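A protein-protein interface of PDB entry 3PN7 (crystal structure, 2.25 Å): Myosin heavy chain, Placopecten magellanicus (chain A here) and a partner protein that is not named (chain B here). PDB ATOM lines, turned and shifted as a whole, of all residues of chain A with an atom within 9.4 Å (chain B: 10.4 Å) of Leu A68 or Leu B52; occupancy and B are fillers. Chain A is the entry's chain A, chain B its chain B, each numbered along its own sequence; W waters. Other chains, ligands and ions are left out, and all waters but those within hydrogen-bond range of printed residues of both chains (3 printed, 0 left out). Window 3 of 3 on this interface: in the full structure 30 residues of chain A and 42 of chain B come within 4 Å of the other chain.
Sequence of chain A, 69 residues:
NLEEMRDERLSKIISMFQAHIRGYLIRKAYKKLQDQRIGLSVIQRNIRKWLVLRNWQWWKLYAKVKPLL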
ATOM      1  N   GLN A  57     -22.017 -24.713 -29.972  1.00  0.00           N
ATOM      2  CA  GLN A  57     -21.594 -24.337 -28.622  1.00  0.00           C
ATOM      3  C   GLN A  57     -20.830 -25.442 -27.876  1.00  0.00           C
ATOM      4  O   GLN A  57     -19.849 -25.164 -27.193  1.00  0.00           O
ATOM      5  CB  GLN A  57     -22.795 -23.864 -27.792  1.00  0.00           C
ATOM      6  CG  GLN A  57     -22.393 -23.371 -26.405  1.00  0.00           C
ATOM      7  CD  GLN A  57     -21.428 -22.197 -26.454  1.00  0.00           C
ATOM      8  OE1 GLN A  57     -20.269 -22.311 -26.031  1.00  0.00           O
ATOM      9  NE2 GLN A  57     -21.896 -21.067 -26.974  1.00  0.00           N
ATOM     10  N   LYS A  60     -17.271 -25.219 -28.964  1.00  0.00           N
ATOM     11  CA  LYS A  60     -16.561 -24.083 -28.383  1.00  0.00           C
ATOM     12  C   LYS A  60     -16.136 -24.361 -26.930  1.00  0.00           C
ATOM     13  O   LYS A  60     -15.020 -24.035 -26.543  1.00  0.00           O
ATOM     14  CB  LYS A  60     -17.375 -22.800 -28.508  1.00  0.00           C
ATOM     15  CG  LYS A  60     -17.410 -22.260 -29.932  1.00  0.00           C
ATOM     16  CD  LYS A  60     -18.804 -21.798 -30.310  1.00  0.00           C
ATOM     17  CE  LYS A  60     -18.873 -20.292 -30.452  1.00  0.00           C
ATOM     18  NZ  LYS A  60     -20.298 -19.841 -30.657  1.00  0.00           N
ATOM     19  N   LEU A  61     -17.019 -24.978 -26.150  1.00  0.00           N
ATOM     20  CA  LEU A  61     -16.662 -25.504 -24.838  1.00  0.00           C
ATOM     21  C   LEU A  61     -15.519 -26.515 -24.969  1.00  0.00           C
ATOM     22  O   LEU A  61     -14.452 -26.356 -24.371  1.00  0.00           O
ATOM     23  CB  LEU A  61     -17.862 -26.194 -24.173  1.00  0.00           C
ATOM     24  CG  LEU A  61     -17.575 -26.719 -22.759  1.00  0.00           C
ATOM     25  CD1 LEU A  61     -16.965 -25.597 -21.935  1.00  0.00           C
ATOM     26  CD2 LEU A  61     -18.814 -27.290 -22.053  1.00  0.00           C
ATOM     27  N   TYR A  62     -15.753 -27.563 -25.749  1.00  0.00           N
ATOM     28  CA  TYR A  62     -14.773 -28.620 -25.882  1.00  0.00           C
ATOM     29  C   TYR A  62     -13.374 -28.054 -26.161  1.00  0.00           C
ATOM     30  O   TYR A  62     -12.394 -28.446 -25.526  1.00  0.00           O
ATOM     31  CB  TYR A  62     -15.208 -29.579 -26.985  1.00  0.00           C
ATOM     32  CG  TYR A  62     -14.428 -30.864 -27.029  1.00  0.00           C
ATOM     33  CD1 TYR A  62     -14.819 -31.965 -26.269  1.00  0.00           C
ATOM     34  CD2 TYR A  62     -13.294 -30.987 -27.841  1.00  0.00           C
ATOM     35  CE1 TYR A  62     -14.106 -33.163 -26.313  1.00  0.00           C
ATOM     36  CE2 TYR A  62     -12.571 -32.182 -27.901  1.00  0.00           C
ATOM     37  CZ  TYR A  62     -12.985 -33.268 -27.136  1.00  0.00           C
ATOM     38  OH  TYR A  62     -12.281 -34.449 -27.191  1.00  0.00           O
ATOM     39  N   ALA A  63     -13.273 -27.113 -27.091  1.00  0.00           N
ATOM     40  CA  ALA A  63     -11.956 -26.604 -27.461  1.00  0.00           C
ATOM     41  C   ALA A  63     -11.302 -25.729 -26.387  1.00  0.00           C
ATOM     42  O   ALA A  63     -10.091 -25.535 -26.416  1.00  0.00           O
ATOM     43  CB  ALA A  63     -12.057 -25.826 -28.764  1.00  0.00           C
ATOM     44  N   LYS A  64     -12.039 -25.195 -25.544  1.00  0.00           N
ATOM     45  CA  LYS A  64     -11.497 -24.487 -24.377  1.00  0.00           C
ATOM     46  C   LYS A  64     -11.045 -25.461 -23.275  1.00  0.00           C
ATOM     47  O   LYS A  64     -10.058 -25.209 -22.580  1.00  0.00           O
ATOM     48  CB  LYS A  64     -12.513 -23.478 -23.809  1.00  0.00           C
ATOM     49  CG  LYS A  64     -12.815 -22.301 -24.730  1.00  0.00           C
ATOM     50  CD  LYS A  64     -13.543 -21.193 -23.981  1.00  0.00           C
ATOM     51  CE  LYS A  64     -13.877 -20.004 -24.878  1.00  0.00           C
ATOM     52  NZ  LYS A  64     -14.643 -18.946 -24.128  1.00  0.00           N
ATOM     53  N   VAL A  65     -11.829 -26.567 -23.030  1.00  0.00           N
ATOM     54  CA  VAL A  65     -11.419 -27.653 -22.134  1.00  0.00           C
ATOM     55  C   VAL A  65     -10.141 -28.387 -22.606  1.00  0.00           C
ATOM     56  O   VAL A  65      -9.327 -28.831 -21.794  1.00  0.00           O
ATOM     57  CB  VAL A  65     -12.568 -28.694 -21.941  1.00  0.00           C
ATOM     58  CG1 VAL A  65     -12.111 -29.869 -21.083  1.00  0.00           C
ATOM     59  CG2 VAL A  65     -13.772 -28.040 -21.324  1.00  0.00           C
ATOM     60  N   LYS A  66      -9.974 -28.507 -23.917  1.00  0.00           N
ATOM     61  CA  LYS A  66      -8.920 -29.334 -24.494  1.00  0.00           C
ATOM     62  C   LYS A  66      -7.504 -29.002 -23.971  1.00  0.00           C
ATOM     63  O   LYS A  66      -6.780 -29.896 -23.543  1.00  0.00           O
ATOM     64  CB  LYS A  66      -8.996 -29.294 -26.034  1.00  0.00           C
ATOM     65  CG  LYS A  66      -8.463 -30.543 -26.760  1.00  0.00           C
ATOM     66  CD  LYS A  66      -8.742 -30.440 -28.276  1.00  0.00           C
ATOM     67  CE  LYS A  66      -8.169 -31.605 -29.112  1.00  0.00           C
ATOM     68  NZ  LYS A  66      -6.701 -31.837 -28.906  1.00  0.00           N
ATOM     69  N   PRO A  67      -7.118 -27.717 -23.977  1.00  0.00           N
ATOM     70  CA  PRO A  67      -5.794 -27.318 -23.475  1.00  0.00           C
ATOM     71  C   PRO A  67      -5.562 -27.629 -21.991  1.00  0.00           C
ATOM     72  O   PRO A  67      -4.412 -27.841 -21.600  1.00  0.00           O
ATOM     73  CB  PRO A  67      -5.777 -25.802 -23.689  1.00  0.00           C
ATOM     74  CG  PRO A  67      -6.798 -25.558 -24.769  1.00  0.00           C
ATOM     75  CD  PRO A  67      -7.871 -26.564 -24.500  1.00  0.00           C
ATOM     76  N   LEU A  68      -6.619 -27.643 -21.180  1.00  0.00           N
ATOM     77  CA  LEU A  68      -6.473 -27.957 -19.760  1.00  0.00           C
ATOM     78  C   LEU A  68      -6.342 -29.464 -19.545  1.00  0.00           C
ATOM     79  O   LEU A  68      -6.156 -29.913 -18.411  1.00  0.00           O
ATOM     80  CB  LEU A  68      -7.668 -27.417 -18.963  1.00  0.00           C
ATOM     81  CG  LEU A  68      -8.213 -26.066 -19.444  1.00  0.00           C
ATOM     82  CD1 LEU A  68      -9.459 -25.663 -18.676  1.00  0.00           C
ATOM     83  CD2 LEU A  68      -7.142 -24.992 -19.331  1.00  0.00           C
ATOM     84  N   LEU A  69      -6.437 -30.211 -20.653  1.00  0.00           N
ATOM     85  CA  LEU A  69      -6.454 -31.685 -20.714  1.00  0.00           C
ATOM     86  C   LEU A  69      -7.886 -32.228 -20.834  1.00  0.00           C
ATOM     87  O   LEU A  69      -8.331 -32.638 -21.915  1.00  0.00           O
ATOM     88  CB  LEU A  69      -5.720 -32.331 -19.527  1.00  0.00           C
ATOM     89  CG  LEU A  69      -4.192 -32.396 -19.511  1.00  0.00           C
ATOM     90  CD1 LEU A  69      -3.674 -33.438 -20.494  1.00  0.00           C
ATOM     91  CD2 LEU A  69      -3.567 -31.032 -19.770  1.00  0.00           C
ATOM     92  N   GLU B  24      -9.355 -38.699 -25.218  1.00  0.00           N
ATOM     93  CA  GLU B  24      -9.542 -37.266 -25.120  1.00  0.00           C
ATOM     94  C   GLU B  24     -10.991 -36.964 -24.707  1.00  0.00           C
ATOM     95  O   GLU B  24     -11.235 -36.186 -23.788  1.00  0.00           O
ATOM     96  CB  GLU B  24      -9.236 -36.644 -26.472  1.00  0.00           C
ATOM     97  CG  GLU B  24      -9.164 -35.135 -26.495  1.00  0.00           C
ATOM     98  CD  GLU B  24      -8.927 -34.633 -27.905  1.00  0.00           C
ATOM     99  OE1 GLU B  24      -7.752 -34.627 -28.342  1.00  0.00           O
ATOM    100  OE2 GLU B  24      -9.917 -34.287 -28.590  1.00  0.00           O
ATOM    101  N   GLU B  27     -11.702 -37.759 -21.121  1.00  0.00           N
ATOM    102  CA  GLU B  27     -11.032 -36.809 -20.244  1.00  0.00           C
ATOM    103  C   GLU B  27     -11.770 -35.478 -20.202  1.00  0.00           C
ATOM    104  O   GLU B  27     -11.879 -34.858 -19.149  1.00  0.00           O
ATOM    105  CB  GLU B  27      -9.578 -36.600 -20.674  1.00  0.00           C
ATOM    106  CG  GLU B  27      -8.559 -37.054 -19.640  1.00  0.00           C
ATOM    107  CD  GLU B  27      -7.257 -36.278 -19.717  1.00  0.00           C
ATOM    108  OE1 GLU B  27      -7.028 -35.408 -18.849  1.00  0.00           O
ATOM    109  OE2 GLU B  27      -6.462 -36.542 -20.642  1.00  0.00           O
ATOM    110  N   ALA B  28     -12.282 -35.048 -21.348  1.00  0.00           N
ATOM    111  CA  ALA B  28     -13.100 -33.836 -21.400  1.00  0.00           C
ATOM    112  C   ALA B  28     -14.399 -34.048 -20.616  1.00  0.00           C
ATOM    113  O   ALA B  28     -14.806 -33.204 -19.815  1.00  0.00           O
ATOM    114  CB  ALA B  28     -13.406 -33.446 -22.850  1.00  0.00           C
ATOM    115  N   THR B  30     -14.928 -36.050 -18.196  1.00  0.00           N
ATOM    116  CA  THR B  30     -14.543 -36.123 -16.796  1.00  0.00           C
ATOM    117  C   THR B  30     -14.357 -34.737 -16.164  1.00  0.00           C
ATOM    118  O   THR B  30     -14.773 -34.504 -15.027  1.00  0.00           O
ATOM    119  CB  THR B  30     -13.264 -37.002 -16.659  1.00  0.00           C
ATOM    120  OG1 THR B  30     -13.607 -38.381 -16.898  1.00  0.00           O
ATOM    121  CG2 THR B  30     -12.599 -36.850 -15.300  1.00  0.00           C
ATOM    122  N   MET B  31     -13.728 -33.821 -16.893  1.00  0.00           N
ATOM    123  CA  MET B  31     -13.508 -32.475 -16.376  1.00  0.00           C
ATOM    124  C   MET B  31     -14.792 -31.648 -16.288  1.00  0.00           C
ATOM    125  O   MET B  31     -14.978 -30.864 -15.354  1.00  0.00           O
ATOM    126  CB  MET B  31     -12.482 -31.725 -17.219  1.00  0.00           C
ATOM    127  CG  MET B  31     -12.173 -30.335 -16.652  1.00  0.00           C
ATOM    128  SD  MET B  31     -10.759 -29.542 -17.453  1.00  0.00           S
ATOM    129  CE  MET B  31      -9.511 -30.796 -17.218  1.00  0.00           C
ATOM    130  N   ILE B  32     -15.674 -31.812 -17.271  1.00  0.00           N
ATOM    131  CA  ILE B  32     -16.921 -31.059 -17.288  1.00  0.00           C
ATOM    132  C   ILE B  32     -17.877 -31.592 -16.220  1.00  0.00           C
ATOM    133  O   ILE B  32     -18.701 -30.849 -15.681  1.00  0.00           O
ATOM    134  CB  ILE B  32     -17.580 -31.081 -18.680  1.00  0.00           C
ATOM    135  CG1 ILE B  32     -16.648 -30.458 -19.713  1.00  0.00           C
ATOM    136  CG2 ILE B  32     -18.869 -30.301 -18.676  1.00  0.00           C
ATOM    137  CD1 ILE B  32     -17.045 -30.782 -21.132  1.00  0.00           C
ATOM    138  N   GLN B  34     -18.103 -31.886 -13.068  1.00  0.00           N
ATOM    139  CA  GLN B  34     -17.546 -31.433 -11.799  1.00  0.00           C
ATOM    140  C   GLN B  34     -18.148 -32.216 -10.613  1.00  0.00           C
ATOM    141  O   GLN B  34     -17.556 -32.292  -9.543  1.00  0.00           O
ATOM    142  CB  GLN B  34     -17.739 -29.916 -11.654  1.00  0.00           C
ATOM    143  CG  GLN B  34     -17.258 -29.084 -12.876  1.00  0.00           C
ATOM    144  CD  GLN B  34     -15.790 -28.616 -12.771  1.00  0.00           C
ATOM    145  OE1 GLN B  34     -14.843 -29.410 -12.920  1.00  0.00           O
ATOM    146  NE2 GLN B  34     -15.605 -27.317 -12.531  1.00  0.00           N
ATOM    147  N   ASP B  44     -23.063 -28.673 -13.621  1.00  0.00           N
ATOM    148  CA  ASP B  44     -21.726 -28.993 -14.118  1.00  0.00           C
ATOM    149  C   ASP B  44     -21.334 -28.042 -15.225  1.00  0.00           C
ATOM    150  O   ASP B  44     -20.215 -27.530 -15.267  1.00  0.00           O
ATOM    151  CB  ASP B  44     -21.695 -30.414 -14.660  1.00  0.00           C
ATOM    152  CG  ASP B  44     -21.662 -31.448 -13.567  1.00  0.00           C
ATOM    153  OD1 ASP B  44     -20.717 -31.409 -12.749  1.00  0.00           O
ATOM    154  OD2 ASP B  44     -22.565 -32.312 -13.537  1.00  0.00           O
ATOM    155  N   LEU B  45     -22.280 -27.808 -16.122  1.00  0.00           N
ATOM    156  CA  LEU B  45     -22.061 -26.956 -17.280  1.00  0.00           C
ATOM    157  C   LEU B  45     -21.829 -25.516 -16.836  1.00  0.00           C
ATOM    158  O   LEU B  45     -20.852 -24.882 -17.258  1.00  0.00           O
ATOM    159  CB  LEU B  45     -23.273 -27.040 -18.211  1.00  0.00           C
ATOM    160  CG  LEU B  45     -23.111 -27.239 -19.717  1.00  0.00           C
ATOM    161  CD1 LEU B  45     -22.040 -28.230 -20.049  1.00  0.00           C
ATOM    162  CD2 LEU B  45     -24.446 -27.666 -20.295  1.00  0.00           C
ATOM    163  N   LYS B  46     -22.724 -25.000 -15.991  1.00  0.00           N
ATOM    164  CA  LYS B  46     -22.561 -23.655 -15.427  1.00  0.00           C
ATOM    165  C   LYS B  46     -21.204 -23.517 -14.744  1.00  0.00           C
ATOM    166  O   LYS B  46     -20.475 -22.541 -14.957  1.00  0.00           O
ATOM    167  CB  LYS B  46     -23.641 -23.360 -14.379  1.00  0.00           C
ATOM    168  CG  LYS B  46     -25.046 -23.180 -14.902  1.00  0.00           C
ATOM    169  CD  LYS B  46     -25.901 -22.458 -13.859  1.00  0.00           C
ATOM    170  CE  LYS B  46     -27.287 -22.142 -14.378  1.00  0.00           C
ATOM    171  NZ  LYS B  46     -27.954 -21.088 -13.556  1.00  0.00           N
ATOM    172  N   GLU B  47     -20.881 -24.500 -13.908  1.00  0.00           N
ATOM    173  CA  GLU B  47     -19.594 -24.540 -13.229  1.00  0.00           C
ATOM    174  C   GLU B  47     -18.433 -24.492 -14.221  1.00  0.00           C
ATOM    175  O   GLU B  47     -17.527 -23.665 -14.088  1.00  0.00           O
ATOM    176  CB  GLU B  47     -19.479 -25.788 -12.350  1.00  0.00           C
ATOM    177  CG  GLU B  47     -18.489 -25.607 -11.237  1.00  0.00           C
ATOM    178  CD  GLU B  47     -18.753 -24.313 -10.459  1.00  0.00           C
ATOM    179  OE1 GLU B  47     -19.925 -24.065 -10.097  1.00  0.00           O
ATOM    180  OE2 GLU B  47     -17.796 -23.534 -10.234  1.00  0.00           O
ATOM    181  N   MET B  48     -18.455 -25.381 -15.213  1.00  0.00           N
ATOM    182  CA  MET B  48     -17.394 -25.396 -16.209  1.00  0.00           C
ATOM    183  C   MET B  48     -17.276 -24.055 -16.931  1.00  0.00           C
ATOM    184  O   MET B  48     -16.178 -23.509 -17.046  1.00  0.00           O
ATOM    185  CB  MET B  48     -17.578 -26.531 -17.211  1.00  0.00           C
ATOM    186  CG  MET B  48     -16.358 -26.735 -18.116  1.00  0.00           C
ATOM    187  SD  MET B  48     -14.934 -27.432 -17.234  1.00  0.00           S
ATOM    188  CE  MET B  48     -13.744 -26.115 -17.381  1.00  0.00           C
ATOM    189  N   PHE B  49     -18.392 -23.512 -17.408  1.00  0.00           N
ATOM    190  CA  PHE B  49     -18.334 -22.242 -18.147  1.00  0.00           C
ATOM    191  C   PHE B  49     -17.783 -21.084 -17.302  1.00  0.00           C
ATOM    192  O   PHE B  49     -16.927 -20.328 -17.773  1.00  0.00           O
ATOM    193  CB  PHE B  49     -19.687 -21.861 -18.777  1.00  0.00           C
ATOM    194  CG  PHE B  49     -19.930 -22.474 -20.153  1.00  0.00           C
ATOM    195  CD1 PHE B  49     -19.215 -22.041 -21.261  1.00  0.00           C
ATOM    196  CD2 PHE B  49     -20.880 -23.472 -20.327  1.00  0.00           C
ATOM    197  CE1 PHE B  49     -19.446 -22.591 -22.522  1.00  0.00           C
ATOM    198  CE2 PHE B  49     -21.114 -24.025 -21.572  1.00  0.00           C
ATOM    199  CZ  PHE B  49     -20.395 -23.586 -22.672  1.00  0.00           C
ATOM    200  N   SER B  50     -18.260 -20.944 -16.065  1.00  0.00           N
ATOM    201  CA  SER B  50     -17.764 -19.862 -15.196  1.00  0.00           C
ATOM    202  C   SER B  50     -16.267 -19.959 -14.919  1.00  0.00           C
ATOM    203  O   SER B  50     -15.600 -18.938 -14.743  1.00  0.00           O
ATOM    204  CB  SER B  50     -18.571 -19.724 -13.888  1.00  0.00           C
ATOM    205  OG  SER B  50     -18.559 -20.904 -13.104  1.00  0.00           O
ATOM    206  N   SER B  51     -15.733 -21.178 -14.913  1.00  0.00           N
ATOM    207  CA  SER B  51     -14.297 -21.360 -14.722  1.00  0.00           C
ATOM    208  C   SER B  51     -13.492 -20.875 -15.920  1.00  0.00           C
ATOM    209  O   SER B  51     -12.285 -20.671 -15.810  1.00  0.00           O
ATOM    210  CB  SER B  51     -13.968 -22.827 -14.442  1.00  0.00           C
ATOM    211  OG  SER B  51     -14.622 -23.280 -13.273  1.00  0.00           O
ATOM    212  N   LEU B  52     -14.157 -20.688 -17.059  1.00  0.00           N
ATOM    213  CA  LEU B  52     -13.471 -20.336 -18.314  1.00  0.00           C
ATOM    214  C   LEU B  52     -13.701 -18.892 -18.764  1.00  0.00           C
ATOM    215  O   LEU B  52     -12.980 -18.382 -19.619  1.00  0.00           O
ATOM    216  CB  LEU B  52     -13.920 -21.260 -19.448  1.00  0.00           C
ATOM    217  CG  LEU B  52     -13.138 -22.520 -19.803  1.00  0.00           C
ATOM    218  CD1 LEU B  52     -11.844 -22.631 -19.025  1.00  0.00           C
ATOM    219  CD2 LEU B  52     -14.000 -23.755 -19.641  1.00  0.00           C
ATOM    220  N   GLY B  53     -14.716 -18.247 -18.205  1.00  0.00           N
ATOM    221  CA  GLY B  53     -15.077 -16.903 -18.612  1.00  0.00           C
ATOM    222  C   GLY B  53     -16.563 -16.652 -18.458  1.00  0.00           C
ATOM    223  O   GLY B  53     -17.153 -17.011 -17.439  1.00  0.00           O
ATOM    224  N   ARG B  54     -17.166 -16.036 -19.474  1.00  0.00           N
ATOM    225  CA  ARG B  54     -18.596 -15.710 -19.464  1.00  0.00           C
ATOM    226  C   ARG B  54     -19.456 -16.965 -19.364  1.00  0.00           C
ATOM    227  O   ARG B  54     -19.232 -17.939 -20.083  1.00  0.00           O
ATOM    228  CB  ARG B  54     -18.967 -14.919 -20.728  1.00  0.00           C
ATOM    229  CG  ARG B  54     -20.442 -14.977 -21.123  1.00  0.00           C
ATOM    230  CD  ARG B  54     -20.604 -14.879 -22.643  1.00  0.00           C
ATOM    231  NE  ARG B  54     -19.891 -13.723 -23.194  1.00  0.00           N
ATOM    232  CZ  ARG B  54     -19.433 -13.636 -24.443  1.00  0.00           C
ATOM    233  NH1 ARG B  54     -19.602 -14.643 -25.295  1.00  0.00           N
ATOM    234  NH2 ARG B  54     -18.796 -12.537 -24.840  1.00  0.00           N
ATOM    235  N   THR B  55     -20.440 -16.948 -18.475  1.00  0.00           N
ATOM    236  CA  THR B  55     -21.328 -18.090 -18.350  1.00  0.00           C
ATOM    237  C   THR B  55     -22.605 -17.856 -19.158  1.00  0.00           C
ATOM    238  O   THR B  55     -23.345 -16.907 -18.897  1.00  0.00           O
ATOM    239  CB  THR B  55     -21.672 -18.387 -16.878  1.00  0.00           C
ATOM    240  OG1 THR B  55     -22.829 -17.643 -16.489  1.00  0.00           O
ATOM    241  CG2 THR B  55     -20.535 -17.998 -15.981  1.00  0.00           C
ATOM    242  N   PRO B  56     -22.857 -18.711 -20.160  1.00  0.00           N
ATOM    243  CA  PRO B  56     -24.101 -18.608 -20.938  1.00  0.00           C
ATOM    244  C   PRO B  56     -25.338 -18.678 -20.031  1.00  0.00           C
ATOM    245  O   PRO B  56     -25.278 -19.249 -18.935  1.00  0.00           O
ATOM    246  CB  PRO B  56     -24.046 -19.837 -21.863  1.00  0.00           C
ATOM    247  CG  PRO B  56     -22.600 -20.178 -21.969  1.00  0.00           C
ATOM    248  CD  PRO B  56     -21.999 -19.817 -20.623  1.00  0.00           C
ATOM    249  N   MET B  64     -28.272 -26.838 -24.802  1.00  0.00           N
ATOM    250  CA  MET B  64     -27.112 -27.713 -25.039  1.00  0.00           C
ATOM    251  C   MET B  64     -27.408 -29.123 -24.572  1.00  0.00           C
ATOM    252  O   MET B  64     -27.129 -30.097 -25.275  1.00  0.00           O
ATOM    253  CB  MET B  64     -25.852 -27.210 -24.329  1.00  0.00           C
ATOM    254  CG  MET B  64     -25.223 -25.957 -24.927  1.00  0.00           C
ATOM    255  SD  MET B  64     -23.739 -25.404 -24.017  1.00  0.00           S
ATOM    256  CE  MET B  64     -22.568 -26.724 -24.364  1.00  0.00           C
ATOM    257  N   SER B 156     -10.705 -21.710 -30.179  1.00  0.00           N
ATOM    258  CA  SER B 156     -12.011 -21.162 -29.821  1.00  0.00           C
ATOM    259  C   SER B 156     -12.770 -22.083 -28.872  1.00  0.00           C
ATOM    260  O   SER B 156     -13.734 -21.668 -28.232  1.00  0.00           O
ATOM    261  CB  SER B 156     -12.848 -20.892 -31.072  1.00  0.00           C
ATOM    262  OG  SER B 156     -13.962 -20.071 -30.768  1.00  0.00           O
HETATM  263  O   HOH W   1     -15.684 -16.142 -22.494  1.00  0.00           O
HETATM  264  O   HOH W   2      -5.900 -33.985 -26.782  1.00  0.00           O
HETATM  265  O   HOH W   3      -6.468 -34.031 -31.006  1.00  0.00           O
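Of the 11 printed residues of chain A, 10 touch a printed residue of chain B.
Printed residues of chain A that touch a printed residue of chain B: Gln A57, Lys A60, Leu A61, Tyr A62, Ala A63, Lys A64, Val A65, Lys A66, Leu A68 and Leu A69.
Hydrophobic or aromatic side chains of chain A that line the printed part of chain B: Leu A61, Tyr A62, Ala A63, Val A65, Leu A68 and Leu A69.
Among the printed residues, Asp or Glu carboxylates within 4 Å of a Lys or Arg side-chain nitrogen of the other chain: Lys A66 with Glu B24 (3.0 Å).
Gln A57 touches Phe B49.
CG of Gln A57 touches SD of Met B64, 3.4 Å away.
Leu B45 touches Leu A61 (CD1 to CD2, 3.9 Å).
CZ of Phe B49 touches CB of Leu A61 (3.9 Å).
Ala B28 touches Tyr A62.
Ala A63 touches Ser B156 (CB to C, 3.8 Å).
Met B31 touches Val A65 (SD to CG1, 3.9 Å).
Met B31 touches Leu A68 (CE to O, 3.7 Å).
CD1 of Leu B52 touches CD1 of Leu A68, 3.9 Å away.
Glu B27 touches Leu A69.
The side-chain amino group of Lys A66 lies within salt-bridge range of the side-chain carboxylate of Glu B24, 3.0 Å away.
O of Lys A60 lies close to O of Ser B156 (3.2 Å).
The side-chain hydroxyl of Tyr A62 is in hydrogen-bond range of the side-chain carboxylate of Glu B24, at 2.8 Å.
OE1 of Gln B34 lies close to O of Met B31 (2.8 Å).
Water W2 bridges the side-chain carboxylate of Glu B24 (2.5 Å) and the side-chain amino group of Lys A66 (3.1 Å).
Water W3 bridges OE1 of Glu B24 (3.0 Å) and NZ of Lys A66 (3.0 Å).
Water W1 bridges the backbone NH of Arg B54 and the side-chain amino group of Lys A64.
Leu A68 touches just these residues of chain B: Met B31 and Leu B52.
Of chain A, only Leu A68 (3.9 Å) comes within 4 Å of Leu B52.
Pro A67 touches none of the printed residues of chain B.
Of chain B, only Glu B27 (3.4 Å) comes within 4 Å of Leu A69.
No residue of chain A comes within 4 Å of Ser B51.
No residue of chain A comes within 4 Å of Gly B53.
Of the printed residues of chain B, Ala A63 touches Ser B156.
Printed residues of chain A within 4 Å of Glu B27: Leu A69 (3.4 Å).
Printed residues of chain B within 4 Å of Gln A57: Phe B49 (3.6 Å) and Met B64 (3.4 Å).
Of the printed residues of chain A, Leu B45 touches Leu A61.
Printed residues of chain A within 4 Å of Ala B28: Tyr A62.
Gln B34 touches none of the printed residues of chain A.
The nearest residue of chain B that does not touch Leu A68 is Met B48 (4.5 Å).
The nearest printed residue of chain B that does not touch Lys A60 is Phe B49 (5.8 Å).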
